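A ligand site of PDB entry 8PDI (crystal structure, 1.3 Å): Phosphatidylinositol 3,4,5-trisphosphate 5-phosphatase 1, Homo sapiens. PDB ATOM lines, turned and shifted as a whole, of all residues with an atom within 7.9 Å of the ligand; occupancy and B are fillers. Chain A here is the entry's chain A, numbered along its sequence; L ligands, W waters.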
ATOM      1  N   SER A 109       6.303  30.964  15.232  1.00  0.00           N
ATOM      2  CA  SER A 109       7.745  30.911  15.368  1.00  0.00           C
ATOM      3  C   SER A 109       8.213  29.458  15.401  1.00  0.00           C
ATOM      4  O   SER A 109       7.395  28.523  15.401  1.00  0.00           O
ATOM      5  CB  SER A 109       8.139  31.691  16.611  1.00  0.00           C
ATOM      6  OG  SER A 109       7.757  30.963  17.767  1.00  0.00           O
ATOM      7  N   HIS A 110       9.519  29.254  15.503  1.00  0.00           N
ATOM      8  CA  HIS A 110      10.097  27.909  15.653  1.00  0.00           C
ATOM      9  C   HIS A 110       9.576  26.971  14.572  1.00  0.00           C
ATOM     10  O   HIS A 110       9.159  25.863  14.876  1.00  0.00           O
ATOM     11  CB  HIS A 110       9.848  27.322  17.052  1.00  0.00           C
ATOM     12  CG  HIS A 110      10.505  28.116  18.186  1.00  0.00           C
ATOM     13  ND1 HIS A 110       9.889  29.180  18.813  1.00  0.00           N
ATOM     14  CD2 HIS A 110      11.700  28.043  18.723  1.00  0.00           C
ATOM     15  CE1 HIS A 110      10.702  29.694  19.743  1.00  0.00           C
ATOM     16  NE2 HIS A 110      11.778  28.926  19.755  1.00  0.00           N
ATOM     17  N   ILE A 111       9.666  27.411  13.334  1.00  0.00           N
ATOM     18  CA  ILE A 111       9.175  26.634  12.228  1.00  0.00           C
ATOM     19  C   ILE A 111      10.207  25.580  11.841  1.00  0.00           C
ATOM     20  O   ILE A 111      11.406  25.861  11.681  1.00  0.00           O
ATOM     21  CB  ILE A 111       8.833  27.533  11.026  1.00  0.00           C
ATOM     22  CG1 ILE A 111       7.762  28.592  11.309  1.00  0.00           C
ATOM     23  CG2 ILE A 111       8.438  26.716   9.818  1.00  0.00           C
ATOM     24  CD1 ILE A 111       7.847  29.757  10.343  1.00  0.00           C
ATOM     25  N   CYS A 112       9.749  24.328  11.728  1.00  0.00           N
ATOM     26  CA  CYS A 112      10.611  23.199  11.373  1.00  0.00           C
ATOM     27  C   CYS A 112       9.974  22.414  10.236  1.00  0.00           C
ATOM     28  O   CYS A 112       8.757  22.305  10.178  1.00  0.00           O
ATOM     29  CB  CYS A 112      10.755  22.181  12.534  1.00  0.00           C
ATOM     30  SG  CYS A 112      10.992  22.819  14.174  1.00  0.00           S
ATOM     31  N   THR A 113      10.812  21.795   9.414  1.00  0.00           N
ATOM     32  CA  THR A 113      10.396  20.884   8.357  1.00  0.00           C
ATOM     33  C   THR A 113      11.298  19.673   8.416  1.00  0.00           C
ATOM     34  O   THR A 113      12.461  19.760   8.777  1.00  0.00           O
ATOM     35  CB  THR A 113      10.392  21.508   6.941  1.00  0.00           C
ATOM     36  OG1 THR A 113      11.727  21.848   6.612  1.00  0.00           O
ATOM     37  CG2 THR A 113       9.548  22.742   6.806  1.00  0.00           C
ATOM     38  N   ASP A 114      10.770  18.544   7.954  1.00  0.00           N
ATOM     39  CA  ASP A 114      11.560  17.331   7.841  1.00  0.00           C
ATOM     40  C   ASP A 114      10.831  16.342   6.925  1.00  0.00           C
ATOM     41  O   ASP A 114       9.653  16.536   6.599  1.00  0.00           O
ATOM     42  CB  ASP A 114      11.845  16.691   9.193  1.00  0.00           C
ATOM     43  CG  ASP A 114      13.002  15.691   9.174  1.00  0.00           C
ATOM     44  OD1 ASP A 114      13.877  15.803   8.257  1.00  0.00           O
ATOM     45  OD2 ASP A 114      13.013  14.798  10.008  1.00  0.00           O
ATOM     46  N   SER A 133       6.307  21.672  11.701  1.00  0.00           N
ATOM     47  CA  SER A 133       5.872  22.073  13.022  1.00  0.00           C
ATOM     48  C   SER A 133       6.161  23.541  13.235  1.00  0.00           C
ATOM     49  O   SER A 133       7.032  24.119  12.573  1.00  0.00           O
ATOM     50  CB  SER A 133       6.465  21.208  14.125  1.00  0.00           C
ATOM     51  OG  SER A 133       7.848  21.438  14.242  1.00  0.00           O
ATOM     52  N   PHE A 134       5.468  24.148  14.207  1.00  0.00           N
ATOM     53  CA  PHE A 134       5.743  25.495  14.623  1.00  0.00           C
ATOM     54  C   PHE A 134       5.027  25.736  15.952  1.00  0.00           C
ATOM     55  O   PHE A 134       4.130  24.983  16.336  1.00  0.00           O
ATOM     56  CB  PHE A 134       5.362  26.545  13.570  1.00  0.00           C
ATOM     57  CG  PHE A 134       3.981  26.460  13.006  1.00  0.00           C
ATOM     58  CD1 PHE A 134       3.743  25.613  11.937  1.00  0.00           C
ATOM     59  CD2 PHE A 134       2.955  27.205  13.540  1.00  0.00           C
ATOM     60  CE1 PHE A 134       2.499  25.569  11.382  1.00  0.00           C
ATOM     61  CE2 PHE A 134       1.682  27.102  13.004  1.00  0.00           C
ATOM     62  CZ  PHE A 134       1.468  26.284  11.886  1.00  0.00           C
ATOM     63  N   MET A 135       5.393  26.833  16.610  1.00  0.00           N
ATOM     64  CA  MET A 135       4.647  27.380  17.730  1.00  0.00           C
ATOM     65  C   MET A 135       3.651  28.418  17.205  1.00  0.00           C
ATOM     66  O   MET A 135       4.020  29.248  16.364  1.00  0.00           O
ATOM     67  CB  MET A 135       5.626  28.090  18.672  1.00  0.00           C
ATOM     68  CG  MET A 135       6.591  27.166  19.396  1.00  0.00           C
ATOM     69  SD  MET A 135       5.854  25.920  20.461  1.00  0.00           S
ATOM     70  CE  MET A 135       5.002  26.971  21.653  1.00  0.00           C
ATOM     71  N   SER A 140       2.090  24.369  20.582  1.00  0.00           N
ATOM     72  CA  SER A 140       2.894  23.688  19.567  1.00  0.00           C
ATOM     73  C   SER A 140       1.981  22.877  18.652  1.00  0.00           C
ATOM     74  O   SER A 140       1.073  22.192  19.088  1.00  0.00           O
ATOM     75  CB  SER A 140       3.932  22.838  20.220  1.00  0.00           C
ATOM     76  OG  SER A 140       3.318  21.907  21.073  1.00  0.00           O
ATOM     77  N   ALA A 170      11.910  14.431  12.536  1.00  0.00           N
ATOM     78  CA  ALA A 170      12.496  15.316  13.530  1.00  0.00           C
ATOM     79  C   ALA A 170      11.847  16.678  13.465  1.00  0.00           C
ATOM     80  O   ALA A 170      12.178  17.495  12.603  1.00  0.00           O
ATOM     81  CB  ALA A 170      14.021  15.398  13.298  1.00  0.00           C
ATOM     82  N   LEU A 171      10.823  16.892  14.320  1.00  0.00           N
ATOM     83  CA  LEU A 171      10.126  18.164  14.375  1.00  0.00           C
ATOM     84  C   LEU A 171      10.019  18.551  15.842  1.00  0.00           C
ATOM     85  O   LEU A 171      10.212  17.719  16.716  1.00  0.00           O
ATOM     86  CB  LEU A 171       8.723  17.968  13.805  1.00  0.00           C
ATOM     87  CG  LEU A 171       8.646  17.619  12.344  1.00  0.00           C
ATOM     88  CD1 LEU A 171       7.229  17.222  12.017  1.00  0.00           C
ATOM     89  CD2 LEU A 171       9.110  18.760  11.431  1.00  0.00           C
ATOM     90  N   GLY A 172       9.655  19.817  16.074  1.00  0.00           N
ATOM     91  CA  GLY A 172       9.404  20.308  17.405  1.00  0.00           C
ATOM     92  C   GLY A 172      10.689  20.557  18.173  1.00  0.00           C
ATOM     93  O   GLY A 172      11.778  20.641  17.607  1.00  0.00           O
ATOM     94  N   ASP A 173      10.510  20.650  19.491  1.00  0.00           N
ATOM     95  CA  ASP A 173      11.585  21.065  20.394  1.00  0.00           C
ATOM     96  C   ASP A 173      12.566  19.906  20.612  1.00  0.00           C
ATOM     97  O   ASP A 173      12.233  18.930  21.241  1.00  0.00           O
ATOM     98  CB  ASP A 173      10.954  21.578  21.686  1.00  0.00           C
ATOM     99  CG  ASP A 173      11.958  22.090  22.707  1.00  0.00           C
ATOM    100  OD1 ASP A 173      13.185  22.053  22.417  1.00  0.00           O
ATOM    101  OD2 ASP A 173      11.489  22.481  23.803  1.00  0.00           O
ATOM    102  N   LYS A 174      13.801  20.075  20.124  1.00  0.00           N
ATOM    103  CA  LYS A 174      14.850  19.074  20.254  1.00  0.00           C
ATOM    104  C   LYS A 174      15.238  18.802  21.702  1.00  0.00           C
ATOM    105  O   LYS A 174      15.788  17.727  22.000  1.00  0.00           O
ATOM    106  CB  LYS A 174      16.125  19.499  19.516  1.00  0.00           C
ATOM    107  CG  LYS A 174      15.913  19.735  18.047  1.00  0.00           C
ATOM    108  CD  LYS A 174      17.178  20.143  17.319  1.00  0.00           C
ATOM    109  CE  LYS A 174      16.847  20.561  15.896  1.00  0.00           C
ATOM    110  NZ  LYS A 174      17.973  21.309  15.277  1.00  0.00           N
ATOM    111  N   LYS A 175      14.900  19.707  22.640  1.00  0.00           N
ATOM    112  CA  LYS A 175      15.152  19.423  24.050  1.00  0.00           C
ATOM    113  C   LYS A 175      14.254  18.316  24.585  1.00  0.00           C
ATOM    114  O   LYS A 175      14.582  17.730  25.625  1.00  0.00           O
ATOM    115  CB  LYS A 175      15.030  20.684  24.896  1.00  0.00           C
ATOM    116  CG  LYS A 175      16.254  21.588  24.732  1.00  0.00           C
ATOM    117  CD  LYS A 175      16.075  22.982  25.283  1.00  0.00           C
ATOM    118  CE  LYS A 175      17.368  23.772  25.201  1.00  0.00           C
ATOM    119  NZ  LYS A 175      17.252  25.060  25.900  1.00  0.00           N
ATOM    120  N   LEU A 176      13.148  18.008  23.872  1.00  0.00           N
ATOM    121  CA  LEU A 176      12.273  16.932  24.285  1.00  0.00           C
ATOM    122  C   LEU A 176      12.832  15.587  23.813  1.00  0.00           C
ATOM    123  O   LEU A 176      12.196  14.863  23.055  1.00  0.00           O
ATOM    124  CB  LEU A 176      10.903  17.226  23.723  1.00  0.00           C
ATOM    125  CG  LEU A 176      10.204  18.497  24.231  1.00  0.00           C
ATOM    126  CD1 LEU A 176       8.835  18.663  23.559  1.00  0.00           C
ATOM    127  CD2 LEU A 176      10.026  18.411  25.733  1.00  0.00           C
ATOM    128  N   ARG A 184       5.291  15.507  21.077  1.00  0.00           N
ATOM    129  CA  ARG A 184       5.922  16.814  21.052  1.00  0.00           C
ATOM    130  C   ARG A 184       5.002  18.003  20.825  1.00  0.00           C
ATOM    131  O   ARG A 184       5.433  19.166  20.965  1.00  0.00           O
ATOM    132  CB  ARG A 184       7.075  16.867  20.039  1.00  0.00           C
ATOM    133  CG  ARG A 184       8.310  16.100  20.506  1.00  0.00           C
ATOM    134  CD  ARG A 184       9.485  16.334  19.537  1.00  0.00           C
ATOM    135  NE  ARG A 184      10.654  15.669  20.072  1.00  0.00           N
ATOM    136  CZ  ARG A 184      11.862  15.783  19.590  1.00  0.00           C
ATOM    137  NH1 ARG A 184      12.105  16.618  18.606  1.00  0.00           N
ATOM    138  NH2 ARG A 184      12.837  15.108  20.147  1.00  0.00           N
ATOM    139  N   PHE A 185       3.720  17.788  20.525  1.00  0.00           N
ATOM    140  CA  PHE A 185       2.832  18.860  20.091  1.00  0.00           C
ATOM    141  C   PHE A 185       1.538  18.871  20.886  1.00  0.00           C
ATOM    142  O   PHE A 185       0.939  17.867  21.131  1.00  0.00           O
ATOM    143  CB  PHE A 185       2.510  18.709  18.608  1.00  0.00           C
ATOM    144  CG  PHE A 185       3.773  18.621  17.785  1.00  0.00           C
ATOM    145  CD1 PHE A 185       4.583  19.714  17.661  1.00  0.00           C
ATOM    146  CD2 PHE A 185       4.177  17.404  17.255  1.00  0.00           C
ATOM    147  CE1 PHE A 185       5.804  19.623  17.023  1.00  0.00           C
ATOM    148  CE2 PHE A 185       5.398  17.323  16.611  1.00  0.00           C
ATOM    149  CZ  PHE A 185       6.197  18.434  16.498  1.00  0.00           C
ATOM    150  N   SER A 361       7.194  23.017  29.177  1.00  0.00           N
ATOM    151  CA  SER A 361       7.331  24.443  28.986  1.00  0.00           C
ATOM    152  C   SER A 361       7.114  25.250  30.255  1.00  0.00           C
ATOM    153  O   SER A 361       7.596  26.382  30.328  1.00  0.00           O
ATOM    154  CB  SER A 361       6.369  24.928  27.918  1.00  0.00           C
ATOM    155  OG  SER A 361       6.704  24.330  26.716  1.00  0.00           O
HETATM  156  C1  LIG L   1      12.693  22.488  14.431  1.00  0.00           C
HETATM  157  C2  LIG L   1      13.016  23.002  15.758  1.00  0.00           C
HETATM  158  N1  LIG L   1      14.122  22.989  16.505  1.00  0.00           N
HETATM  159  N2  LIG L   1      13.876  23.544  17.749  1.00  0.00           N
HETATM  160  C3  LIG L   1      12.620  23.907  17.901  1.00  0.00           C
HETATM  161  C4  LIG L   1      11.912  24.395  19.077  1.00  0.00           C
HETATM  162  C5  LIG L   1      10.515  24.277  19.102  1.00  0.00           C
HETATM  163  C6  LIG L   1       9.769  24.770  20.174  1.00  0.00           C
HETATM  164  C7  LIG L   1      10.402  25.406  21.188  1.00  0.00           C
HETATM  165  C8  LIG L   1      11.778  25.545  21.158  1.00  0.00           C
HETATM  166  C9  LIG L   1      12.551  25.065  20.107  1.00  0.00           C
HETATM  167  S1  LIG L   1      11.688  23.770  16.537  1.00  0.00           S
HETATM  168  N3  LIG L   1      13.461  22.621  13.377  1.00  0.00           N
HETATM  169  O   HOH W   1      14.953  23.914  22.254  1.00  0.00           O
HETATM  170  O   HOH W   2      13.625  22.515  10.194  1.00  0.00           O
HETATM  171  O   HOH W   3      13.238  26.307  16.154  1.00  0.00           O
HETATM  172  O   HOH W   4       8.416  23.439  16.059  1.00  0.00           O
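The side-chain sulfur (SG) of Cys 112 is bonded to a carbon (C1) of the ligand.
O of Gly 172 sits close to N1 of the ligand, 3.5 Å away.
The backbone NH (N) of Gly 172 lies within hydrogen-bond range of the side-chain sulfur (SG) of Cys 112, at 3.8 Å.
N of Cys 112 is in hydrogen-bond range of O of Ser 133, at 2.9 Å.
N of Gly 172 sits at hydrogen-bond distance from OG of Ser 133 (3.0 Å).
ND1 of His 110 lies within hydrogen-bond range of OG of Ser 109 (3.0 Å).
OD1 of Asp 173 sits at hydrogen-bond distance from N of Lys 175, at 2.9 Å.
The backbone carbonyl oxygen (O) of His 110 lies close to a sulfur (S1) of the ligand.
Residues that only touch the ligand: Asp 173 and Lys 174.
Hydrophobic or aromatic side chains that line the ligand: His 110.
Of the 20 residues printed, 5 come within 4 Å of the ligand.
The nearest printed residue that does not touch the ligand is Met 135 (4.1 Å).
Water W2 lies within hydrogen-bond range of the backbone NH of Thr 113 (3.0 Å) and a nitrogen (N3) of the ligand (3.2 Å).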
